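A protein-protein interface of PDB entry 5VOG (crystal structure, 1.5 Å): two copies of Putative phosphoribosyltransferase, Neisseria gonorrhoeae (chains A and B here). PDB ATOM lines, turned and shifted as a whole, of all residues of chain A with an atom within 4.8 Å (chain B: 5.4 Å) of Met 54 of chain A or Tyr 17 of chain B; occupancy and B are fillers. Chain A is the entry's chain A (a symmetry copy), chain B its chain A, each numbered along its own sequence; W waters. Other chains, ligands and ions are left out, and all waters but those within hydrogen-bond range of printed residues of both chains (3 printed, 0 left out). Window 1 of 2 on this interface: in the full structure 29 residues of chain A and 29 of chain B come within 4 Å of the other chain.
Among the printed residues, pairs that only touch across the chains: Tyr 17 of chain A with Tyr 17 of chain B (3.3 Å), Tyr 17 of chain A with Asp 18 of chain B (3.4 Å), Tyr 17 of chain A with Met 54 of chain B (3.4 Å), Asp 18 of chain A with Tyr 17 of chain B (3.4 Å), Asp 18 of chain A with Ile 171 of chain B (3.5 Å), His 21 of chain A with Pro 165 of chain B (3.2 Å), His 21 of chain A with Ile 171 of chain B (3.7 Å), Arg 53 of chain A with Ile 50 of chain B (3.6 Å) and Met 54 of chain A with Tyr 17 of chain B (3.4 Å).
Tyr 17 of chain B touches its own counterpart, Tyr 17 of chain A.
Tyr 17 of chain A touches Asp 18 of chain B, and with the chains exchanged Asp 18 of chain A touches Tyr 17 of chain B.
Tyr 17 of chain A touches His 21 of chain B, and with the chains exchanged His 21 of chain A touches Tyr 17 of chain B.
Tyr 17 of chain A touches Met 54 of chain B, and with the chains exchanged Met 54 of chain A touches Tyr 17 of chain B.
6 positions are printed for both chains.
Of the 14 pairs that touch across the chains among the printed residues, 7 have their exchanged pair printed and touching as well.
The backbone carbonyl oxygen (O) of Ile 171 of chain B lies close to the side-chain amide nitrogen (ND2) of Asn 175 of chain B (3.3 Å).
OG1 of Thr 16 of chain B lies close to N of Asp 18 of chain B (3.4 Å).
Water W2 bridges OD1 of Asp 18 of chain B and N of Tyr 17 of chain A.
Water W3 lies within hydrogen-bond range of the side-chain carboxylate (OD1) of Asp 18 of chain A (2.7 Å), the side-chain amide oxygen (OD1) of Asn 175 of chain B (2.7 Å) and the backbone NH (N) of Tyr 17 of chain B (3.0 Å).
Water W1 lies within hydrogen-bond range of N of Ile 171 of chain B and NE2 of His 21 of chain A.
The side-chain amide nitrogen (ND2) of Asn 175 of chain B sits at hydrogen-bond distance from the side-chain carboxylate (OD2) of Asp 18 of chain A (2.8 Å).
ND1 of His 21 of chain B sits at hydrogen-bond distance from OH of Tyr 17 of chain A.
The side-chain hydroxyl of Tyr 17 of chain B sits at hydrogen-bond distance from a ring nitrogen (ND1) of His 21 of chain A (2.7 Å).
The backbone carbonyl oxygen (O) of Trp 166 of chain B is in hydrogen-bond range of the guanidinium group (NH1) of Arg 53 of chain A (3.1 Å).
The backbone carbonyl oxygen (O) of Trp 166 of chain B lies close to the side-chain sulfur (SG) of Cys 57 of chain A (3.8 Å).
Hydrophobic or aromatic side chains of chain B within 4 Å of the printed part of chain A: Tyr 17, His 21, Ile 50, Met 54, Trp 166 and Ile 171.
Hydrophobic or aromatic side chains of chain A within 4 Å of the printed part of chain B: Tyr 17, His 21 and Met 54.
Along chain A the printed residues that touch a printed residue of chain B span positions 17 to 57.
Of chain B, only Tyr 17 comes within 4 Å of Met 54 of chain A.
Tyr 17 of chain B touches four residues of chain A.
Of the printed residues of chain A, Met 54 of chain B touches Tyr 17 (3.4 Å).
Of the printed residues of chain A, Asn 175 of chain B touches Asp 18 (2.8 Å).
The nearest printed residue of chain A that does not touch Tyr 17 of chain B is Ile 50 of chain A (5.6 Å).
The nearest printed residue of chain A that does not touch His 21 of chain B is Ile 50 of chain A (7.6 Å).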
ATOM      1  N   TYR A  17     -13.571 -20.668  24.418  1.00  0.00           N
ATOM      2  CA  TYR A  17     -12.278 -21.185  24.858  1.00  0.00           C
ATOM      3  C   TYR A  17     -11.914 -22.453  24.101  1.00  0.00           C
ATOM      4  O   TYR A  17     -10.773 -22.616  23.661  1.00  0.00           O
ATOM      5  CB  TYR A  17     -12.287 -21.475  26.360  1.00  0.00           C
ATOM      6  CG  TYR A  17     -12.124 -20.276  27.270  1.00  0.00           C
ATOM      7  CD1 TYR A  17     -10.904 -19.606  27.365  1.00  0.00           C
ATOM      8  CD2 TYR A  17     -13.174 -19.843  28.077  1.00  0.00           C
ATOM      9  CE1 TYR A  17     -10.749 -18.513  28.206  1.00  0.00           C
ATOM     10  CE2 TYR A  17     -13.026 -18.754  28.927  1.00  0.00           C
ATOM     11  CZ  TYR A  17     -11.813 -18.093  28.990  1.00  0.00           C
ATOM     12  OH  TYR A  17     -11.660 -17.008  29.836  1.00  0.00           O
ATOM     13  N   ASP A  18     -12.880 -23.363  23.935  1.00  0.00           N
ATOM     14  CA  ASP A  18     -12.602 -24.621  23.247  1.00  0.00           C
ATOM     15  C   ASP A  18     -12.278 -24.398  21.774  1.00  0.00           C
ATOM     16  O   ASP A  18     -11.408 -25.083  21.222  1.00  0.00           O
ATOM     17  CB  ASP A  18     -13.786 -25.572  23.376  1.00  0.00           C
ATOM     18  CG  ASP A  18     -13.953 -26.131  24.785  1.00  0.00           C
ATOM     19  OD1 ASP A  18     -13.067 -25.911  25.636  1.00  0.00           O
ATOM     20  OD2 ASP A  18     -14.978 -26.795  25.043  1.00  0.00           O
ATOM     21  N   ILE A  20     -10.674 -21.961  20.571  1.00  0.00           N
ATOM     22  CA  ILE A  20      -9.297 -21.493  20.510  1.00  0.00           C
ATOM     23  C   ILE A  20      -8.333 -22.626  20.825  1.00  0.00           C
ATOM     24  O   ILE A  20      -7.302 -22.785  20.160  1.00  0.00           O
ATOM     25  CB  ILE A  20      -9.142 -20.290  21.460  1.00  0.00           C
ATOM     26  CG1 ILE A  20      -9.864 -19.089  20.822  1.00  0.00           C
ATOM     27  CG2 ILE A  20      -7.666 -20.005  21.795  1.00  0.00           C
ATOM     28  CD1 ILE A  20     -10.028 -17.898  21.748  1.00  0.00           C
ATOM     29  N   HIS A  21      -8.669 -23.452  21.822  1.00  0.00           N
ATOM     30  CA  HIS A  21      -7.867 -24.632  22.138  1.00  0.00           C
ATOM     31  C   HIS A  21      -7.663 -25.516  20.908  1.00  0.00           C
ATOM     32  O   HIS A  21      -6.543 -25.979  20.650  1.00  0.00           O
ATOM     33  CB  HIS A  21      -8.550 -25.409  23.270  1.00  0.00           C
ATOM     34  CG  HIS A  21      -7.758 -26.571  23.789  1.00  0.00           C
ATOM     35  ND1 HIS A  21      -7.065 -26.526  24.980  1.00  0.00           N
ATOM     36  CD2 HIS A  21      -7.570 -27.816  23.290  1.00  0.00           C
ATOM     37  CE1 HIS A  21      -6.479 -27.693  25.189  1.00  0.00           C
ATOM     38  NE2 HIS A  21      -6.772 -28.494  24.178  1.00  0.00           N
ATOM     39  N   ILE A  24      -5.167 -23.917  18.607  1.00  0.00           N
ATOM     40  CA  ILE A  24      -3.816 -24.032  19.154  1.00  0.00           C
ATOM     41  C   ILE A  24      -3.236 -25.423  18.896  1.00  0.00           C
ATOM     42  O   ILE A  24      -2.052 -25.563  18.564  1.00  0.00           O
ATOM     43  CB  ILE A  24      -3.817 -23.687  20.655  1.00  0.00           C
ATOM     44  CG1 ILE A  24      -4.142 -22.206  20.885  1.00  0.00           C
ATOM     45  CG2 ILE A  24      -2.479 -24.057  21.284  1.00  0.00           C
ATOM     46  CD1 ILE A  24      -3.030 -21.246  20.426  1.00  0.00           C
ATOM     47  N   ILE A  50      -2.557 -16.729  27.381  1.00  0.00           N
ATOM     48  CA  ILE A  50      -3.425 -17.904  27.289  1.00  0.00           C
ATOM     49  C   ILE A  50      -3.041 -18.737  26.065  1.00  0.00           C
ATOM     50  O   ILE A  50      -2.856 -19.952  26.202  1.00  0.00           O
ATOM     51  CB  ILE A  50      -4.912 -17.509  27.313  1.00  0.00           C
ATOM     52  CG1 ILE A  50      -5.233 -16.851  28.667  1.00  0.00           C
ATOM     53  CG2 ILE A  50      -5.779 -18.739  27.094  1.00  0.00           C
ATOM     54  CD1 ILE A  50      -6.674 -16.441  28.851  1.00  0.00           C
ATOM     55  N   PRO A  51      -2.867 -18.156  24.869  1.00  0.00           N
ATOM     56  CA  PRO A  51      -2.335 -18.963  23.749  1.00  0.00           C
ATOM     57  C   PRO A  51      -1.039 -19.698  24.069  1.00  0.00           C
ATOM     58  O   PRO A  51      -0.891 -20.866  23.674  1.00  0.00           O
ATOM     59  CB  PRO A  51      -2.140 -17.917  22.645  1.00  0.00           C
ATOM     60  CG  PRO A  51      -3.209 -16.920  22.908  1.00  0.00           C
ATOM     61  CD  PRO A  51      -3.215 -16.792  24.428  1.00  0.00           C
ATOM     62  N   ALA A  52      -0.104 -19.060  24.791  1.00  0.00           N
ATOM     63  CA  ALA A  52       1.165 -19.725  25.095  1.00  0.00           C
ATOM     64  C   ALA A  52       0.966 -20.914  26.028  1.00  0.00           C
ATOM     65  O   ALA A  52       1.570 -21.974  25.823  1.00  0.00           O
ATOM     66  CB  ALA A  52       2.167 -18.735  25.694  1.00  0.00           C
ATOM     67  N   ARG A  53       0.142 -20.766  27.073  1.00  0.00           N
ATOM     68  CA  ARG A  53      -0.035 -21.900  27.978  1.00  0.00           C
ATOM     69  C   ARG A  53      -0.827 -23.021  27.310  1.00  0.00           C
ATOM     70  O   ARG A  53      -0.541 -24.203  27.551  1.00  0.00           O
ATOM     71  CB  ARG A  53      -0.698 -21.455  29.284  1.00  0.00           C
ATOM     72  CG  ARG A  53      -0.900 -22.606  30.286  1.00  0.00           C
ATOM     73  CD  ARG A  53       0.418 -23.294  30.640  1.00  0.00           C
ATOM     74  NE  ARG A  53       0.268 -24.458  31.519  1.00  0.00           N
ATOM     75  CZ  ARG A  53      -0.078 -25.674  31.109  1.00  0.00           C
ATOM     76  NH1 ARG A  53      -0.335 -25.913  29.821  1.00  0.00           N
ATOM     77  NH2 ARG A  53      -0.164 -26.664  31.992  1.00  0.00           N
ATOM     78  N   MET A  54      -1.784 -22.683  26.434  1.00  0.00           N
ATOM     79  CA  MET A  54      -2.421 -23.723  25.630  1.00  0.00           C
ATOM     80  C   MET A  54      -1.399 -24.419  24.739  1.00  0.00           C
ATOM     81  O   MET A  54      -1.401 -25.650  24.611  1.00  0.00           O
ATOM     82  CB  MET A  54      -3.548 -23.129  24.778  1.00  0.00           C
ATOM     83  CG  MET A  54      -4.779 -22.686  25.567  1.00  0.00           C
ATOM     84  SD  MET A  54      -5.927 -21.920  24.397  1.00  0.00           S
ATOM     85  CE  MET A  54      -7.406 -21.776  25.401  1.00  0.00           C
ATOM     86  N   LEU A  55      -0.506 -23.641  24.120  1.00  0.00           N
ATOM     87  CA  LEU A  55       0.512 -24.235  23.266  1.00  0.00           C
ATOM     88  C   LEU A  55       1.454 -25.142  24.053  1.00  0.00           C
ATOM     89  O   LEU A  55       1.969 -26.120  23.506  1.00  0.00           O
ATOM     90  CB  LEU A  55       1.276 -23.122  22.560  1.00  0.00           C
ATOM     91  CG  LEU A  55       2.115 -23.479  21.344  1.00  0.00           C
ATOM     92  CD1 LEU A  55       1.315 -24.256  20.290  1.00  0.00           C
ATOM     93  CD2 LEU A  55       2.696 -22.198  20.759  1.00  0.00           C
ATOM     94  N   ARG A  56       1.686 -24.842  25.341  1.00  0.00           N
ATOM     95  CA  ARG A  56       2.591 -25.682  26.125  1.00  0.00           C
ATOM     96  C   ARG A  56       2.062 -27.100  26.264  1.00  0.00           C
ATOM     97  O   ARG A  56       2.847 -28.043  26.410  1.00  0.00           O
ATOM     98  CB  ARG A  56       2.836 -25.078  27.510  1.00  0.00           C
ATOM     99  CG  ARG A  56       4.151 -25.513  28.124  1.00  0.00           C
ATOM    100  CD  ARG A  56       4.329 -24.968  29.536  1.00  0.00           C
ATOM    101  NE  ARG A  56       3.677 -25.824  30.522  1.00  0.00           N
ATOM    102  CZ  ARG A  56       3.729 -25.634  31.838  1.00  0.00           C
ATOM    103  NH1 ARG A  56       4.368 -24.589  32.344  1.00  0.00           N
ATOM    104  NH2 ARG A  56       3.117 -26.484  32.651  1.00  0.00           N
ATOM    105  N   CYS A  57       0.738 -27.267  26.220  1.00  0.00           N
ATOM    106  CA  CYS A  57       0.150 -28.601  26.256  1.00  0.00           C
ATOM    107  C   CYS A  57       0.712 -29.475  25.146  1.00  0.00           C
ATOM    108  O   CYS A  57       0.935 -30.679  25.336  1.00  0.00           O
ATOM    109  CB  CYS A  57      -1.366 -28.490  26.123  1.00  0.00           C
ATOM    110  SG  CYS A  57      -2.238 -30.044  26.198  1.00  0.00           S
ATOM    111  N   PHE A  58       0.965 -28.877  23.984  1.00  0.00           N
ATOM    112  CA  PHE A  58       1.378 -29.607  22.800  1.00  0.00           C
ATOM    113  C   PHE A  58       2.864 -29.500  22.501  1.00  0.00           C
ATOM    114  O   PHE A  58       3.422 -30.425  21.911  1.00  0.00           O
ATOM    115  CB  PHE A  58       0.565 -29.116  21.601  1.00  0.00           C
ATOM    116  CG  PHE A  58      -0.916 -29.230  21.815  1.00  0.00           C
ATOM    117  CD1 PHE A  58      -1.554 -30.454  21.668  1.00  0.00           C
ATOM    118  CD2 PHE A  58      -1.667 -28.127  22.193  1.00  0.00           C
ATOM    119  CE1 PHE A  58      -2.914 -30.572  21.895  1.00  0.00           C
ATOM    120  CE2 PHE A  58      -3.025 -28.240  22.423  1.00  0.00           C
ATOM    121  CZ  PHE A  58      -3.651 -29.463  22.266  1.00  0.00           C
ATOM    122  N   TYR B  15     -12.179 -30.012  34.983  1.00  0.00           N
ATOM    123  CA  TYR B  15     -12.884 -28.743  34.883  1.00  0.00           C
ATOM    124  C   TYR B  15     -12.777 -28.213  33.463  1.00  0.00           C
ATOM    125  O   TYR B  15     -11.697 -28.237  32.868  1.00  0.00           O
ATOM    126  CB  TYR B  15     -12.312 -27.688  35.847  1.00  0.00           C
ATOM    127  CG  TYR B  15     -12.494 -27.980  37.316  1.00  0.00           C
ATOM    128  CD1 TYR B  15     -13.763 -28.094  37.879  1.00  0.00           C
ATOM    129  CD2 TYR B  15     -11.393 -28.103  38.154  1.00  0.00           C
ATOM    130  CE1 TYR B  15     -13.920 -28.344  39.232  1.00  0.00           C
ATOM    131  CE2 TYR B  15     -11.542 -28.345  39.509  1.00  0.00           C
ATOM    132  CZ  TYR B  15     -12.802 -28.469  40.041  1.00  0.00           C
ATOM    133  OH  TYR B  15     -12.937 -28.706  41.394  1.00  0.00           O
ATOM    134  N   THR B  16     -13.890 -27.717  32.930  1.00  0.00           N
ATOM    135  CA  THR B  16     -13.854 -27.074  31.626  1.00  0.00           C
ATOM    136  C   THR B  16     -13.247 -25.677  31.746  1.00  0.00           C
ATOM    137  O   THR B  16     -13.142 -25.108  32.834  1.00  0.00           O
ATOM    138  CB  THR B  16     -15.260 -26.974  31.017  1.00  0.00           C
ATOM    139  OG1 THR B  16     -16.047 -26.047  31.778  1.00  0.00           O
ATOM    140  CG2 THR B  16     -15.953 -28.338  30.994  1.00  0.00           C
ATOM    141  N   TYR B  17     -12.841 -25.119  30.599  1.00  0.00           N
ATOM    142  CA  TYR B  17     -12.410 -23.724  30.588  1.00  0.00           C
ATOM    143  C   TYR B  17     -13.486 -22.819  31.168  1.00  0.00           C
ATOM    144  O   TYR B  17     -13.192 -21.924  31.965  1.00  0.00           O
ATOM    145  CB  TYR B  17     -12.073 -23.267  29.169  1.00  0.00           C
ATOM    146  CG  TYR B  17     -10.722 -23.695  28.635  1.00  0.00           C
ATOM    147  CD1 TYR B  17      -9.543 -23.142  29.137  1.00  0.00           C
ATOM    148  CD2 TYR B  17     -10.624 -24.612  27.591  1.00  0.00           C
ATOM    149  CE1 TYR B  17      -8.304 -23.525  28.642  1.00  0.00           C
ATOM    150  CE2 TYR B  17      -9.387 -24.996  27.085  1.00  0.00           C
ATOM    151  CZ  TYR B  17      -8.232 -24.451  27.612  1.00  0.00           C
ATOM    152  OH  TYR B  17      -6.998 -24.829  27.110  1.00  0.00           O
ATOM    153  N   ASP B  18     -14.746 -23.042  30.781  1.00  0.00           N
ATOM    154  CA  ASP B  18     -15.833 -22.196  31.268  1.00  0.00           C
ATOM    155  C   ASP B  18     -16.048 -22.365  32.767  1.00  0.00           C
ATOM    156  O   ASP B  18     -16.338 -21.383  33.464  1.00  0.00           O
ATOM    157  CB  ASP B  18     -17.126 -22.507  30.522  1.00  0.00           C
ATOM    158  CG  ASP B  18     -17.111 -22.026  29.075  1.00  0.00           C
ATOM    159  OD1 ASP B  18     -16.166 -21.313  28.680  1.00  0.00           O
ATOM    160  OD2 ASP B  18     -18.053 -22.364  28.328  1.00  0.00           O
ATOM    161  N   ASP B  19     -15.945 -23.601  33.277  1.00  0.00           N
ATOM    162  CA  ASP B  19     -16.008 -23.819  34.723  1.00  0.00           C
ATOM    163  C   ASP B  19     -15.026 -22.905  35.442  1.00  0.00           C
ATOM    164  O   ASP B  19     -15.354 -22.274  36.454  1.00  0.00           O
ATOM    165  CB  ASP B  19     -15.672 -25.273  35.085  1.00  0.00           C
ATOM    166  CG  ASP B  19     -16.752 -26.270  34.709  1.00  0.00           C
ATOM    167  OD1 ASP B  19     -17.954 -25.917  34.656  1.00  0.00           O
ATOM    168  OD2 ASP B  19     -16.371 -27.445  34.504  1.00  0.00           O
ATOM    169  N   ILE B  20     -13.799 -22.839  34.929  1.00  0.00           N
ATOM    170  CA  ILE B  20     -12.754 -22.073  35.592  1.00  0.00           C
ATOM    171  C   ILE B  20     -13.013 -20.581  35.452  1.00  0.00           C
ATOM    172  O   ILE B  20     -12.857 -19.817  36.413  1.00  0.00           O
ATOM    173  CB  ILE B  20     -11.389 -22.501  35.021  1.00  0.00           C
ATOM    174  CG1 ILE B  20     -11.074 -23.909  35.558  1.00  0.00           C
ATOM    175  CG2 ILE B  20     -10.285 -21.472  35.327  1.00  0.00           C
ATOM    176  CD1 ILE B  20      -9.892 -24.581  34.884  1.00  0.00           C
ATOM    177  N   HIS B  21     -13.448 -20.147  34.264  1.00  0.00           N
ATOM    178  CA  HIS B  21     -13.827 -18.752  34.054  1.00  0.00           C
ATOM    179  C   HIS B  21     -14.866 -18.293  35.075  1.00  0.00           C
ATOM    180  O   HIS B  21     -14.746 -17.198  35.642  1.00  0.00           O
ATOM    181  CB  HIS B  21     -14.350 -18.589  32.621  1.00  0.00           C
ATOM    182  CG  HIS B  21     -14.644 -17.174  32.226  1.00  0.00           C
ATOM    183  ND1 HIS B  21     -13.805 -16.437  31.416  1.00  0.00           N
ATOM    184  CD2 HIS B  21     -15.695 -16.368  32.510  1.00  0.00           C
ATOM    185  CE1 HIS B  21     -14.326 -15.238  31.224  1.00  0.00           C
ATOM    186  NE2 HIS B  21     -15.474 -15.171  31.876  1.00  0.00           N
ATOM    187  N   ARG B  22     -15.878 -19.129  35.346  1.00  0.00           N
ATOM    188  CA  ARG B  22     -16.913 -18.761  36.313  1.00  0.00           C
ATOM    189  C   ARG B  22     -16.340 -18.628  37.721  1.00  0.00           C
ATOM    190  O   ARG B  22     -16.745 -17.739  38.483  1.00  0.00           O
ATOM    191  CB  ARG B  22     -18.044 -19.792  36.287  1.00  0.00           C
ATOM    192  CG  ARG B  22     -18.757 -19.916  34.947  1.00  0.00           C
ATOM    193  CD  ARG B  22     -19.754 -21.069  34.940  1.00  0.00           C
ATOM    194  NE  ARG B  22     -20.192 -21.399  33.583  1.00  0.00           N
ATOM    195  CZ  ARG B  22     -21.214 -20.817  32.962  1.00  0.00           C
ATOM    196  NH1 ARG B  22     -21.915 -19.870  33.573  1.00  0.00           N
ATOM    197  NH2 ARG B  22     -21.538 -21.181  31.728  1.00  0.00           N
ATOM    198  N   ILE B  50      -3.033 -18.451  32.816  1.00  0.00           N
ATOM    199  CA  ILE B  50      -4.419 -18.423  32.348  1.00  0.00           C
ATOM    200  C   ILE B  50      -5.325 -17.857  33.442  1.00  0.00           C
ATOM    201  O   ILE B  50      -6.115 -16.951  33.155  1.00  0.00           O
ATOM    202  CB  ILE B  50      -4.868 -19.806  31.842  1.00  0.00           C
ATOM    203  CG1 ILE B  50      -4.016 -20.193  30.620  1.00  0.00           C
ATOM    204  CG2 ILE B  50      -6.345 -19.769  31.478  1.00  0.00           C
ATOM    205  CD1 ILE B  50      -4.371 -21.518  29.989  1.00  0.00           C
ATOM    206  N   MET B  54      -7.582 -14.421  32.824  1.00  0.00           N
ATOM    207  CA  MET B  54      -9.014 -14.435  33.114  1.00  0.00           C
ATOM    208  C   MET B  54      -9.361 -13.395  34.172  1.00  0.00           C
ATOM    209  O   MET B  54     -10.360 -12.674  34.051  1.00  0.00           O
ATOM    210  CB  MET B  54      -9.456 -15.827  33.575  1.00  0.00           C
ATOM    211  CG  MET B  54      -9.449 -16.895  32.481  1.00  0.00           C
ATOM    212  SD  MET B  54      -9.889 -18.469  33.257  1.00  0.00           S
ATOM    213  CE  MET B  54     -10.159 -19.505  31.817  1.00  0.00           C
ATOM    214  N   PRO B 165      -8.089 -27.961  31.755  1.00  0.00           N
ATOM    215  CA  PRO B 165      -8.348 -28.047  30.310  1.00  0.00           C
ATOM    216  C   PRO B 165      -7.137 -27.673  29.472  1.00  0.00           C
ATOM    217  O   PRO B 165      -7.010 -28.138  28.331  1.00  0.00           O
ATOM    218  CB  PRO B 165      -9.513 -27.067  30.108  1.00  0.00           C
ATOM    219  CG  PRO B 165      -9.376 -26.074  31.238  1.00  0.00           C
ATOM    220  CD  PRO B 165      -8.849 -26.876  32.406  1.00  0.00           C
ATOM    221  N   TRP B 166      -6.242 -26.848  30.006  1.00  0.00           N
ATOM    222  CA  TRP B 166      -5.046 -26.459  29.274  1.00  0.00           C
ATOM    223  C   TRP B 166      -3.976 -27.540  29.281  1.00  0.00           C
ATOM    224  O   TRP B 166      -2.882 -27.313  28.753  1.00  0.00           O
ATOM    225  CB  TRP B 166      -4.495 -25.149  29.833  1.00  0.00           C
ATOM    226  CG  TRP B 166      -4.358 -25.040  31.344  1.00  0.00           C
ATOM    227  CD1 TRP B 166      -3.371 -25.582  32.122  1.00  0.00           C
ATOM    228  CD2 TRP B 166      -5.197 -24.280  32.234  1.00  0.00           C
ATOM    229  NE1 TRP B 166      -3.551 -25.213  33.440  1.00  0.00           N
ATOM    230  CE2 TRP B 166      -4.664 -24.419  33.533  1.00  0.00           C
ATOM    231  CE3 TRP B 166      -6.350 -23.508  32.057  1.00  0.00           C
ATOM    232  CZ2 TRP B 166      -5.234 -23.798  34.645  1.00  0.00           C
ATOM    233  CZ3 TRP B 166      -6.918 -22.894  33.163  1.00  0.00           C
ATOM    234  CH2 TRP B 166      -6.365 -23.054  34.443  1.00  0.00           C
ATOM    235  N   ILE B 171      -9.655 -32.072  23.894  1.00  0.00           N
ATOM    236  CA  ILE B 171     -10.544 -31.254  24.718  1.00  0.00           C
ATOM    237  C   ILE B 171     -11.952 -31.846  24.763  1.00  0.00           C
ATOM    238  O   ILE B 171     -12.681 -31.651  25.745  1.00  0.00           O
ATOM    239  CB  ILE B 171     -10.541 -29.794  24.220  1.00  0.00           C
ATOM    240  CG1 ILE B 171     -11.221 -28.855  25.225  1.00  0.00           C
ATOM    241  CG2 ILE B 171     -11.194 -29.680  22.845  1.00  0.00           C
ATOM    242  CD1 ILE B 171     -10.523 -28.747  26.589  1.00  0.00           C
ATOM    243  N   ASN B 175     -13.750 -32.633  28.219  1.00  0.00           N
ATOM    244  CA  ASN B 175     -15.055 -32.103  28.590  1.00  0.00           C
ATOM    245  C   ASN B 175     -16.013 -33.220  28.972  1.00  0.00           C
ATOM    246  O   ASN B 175     -16.846 -33.048  29.869  1.00  0.00           O
ATOM    247  CB  ASN B 175     -15.642 -31.273  27.450  1.00  0.00           C
ATOM    248  CG  ASN B 175     -14.941 -29.938  27.273  1.00  0.00           C
ATOM    249  OD1 ASN B 175     -14.299 -29.419  28.196  1.00  0.00           O
ATOM    250  ND2 ASN B 175     -15.068 -29.367  26.081  1.00  0.00           N
HETATM  251  O   HOH W   1      -7.857 -30.795  21.939  1.00  0.00           O
HETATM  252  O   HOH W   2     -16.103 -20.533  26.073  1.00  0.00           O
HETATM  253  O   HOH W   3     -13.414 -26.836  28.172  1.00  0.00           O
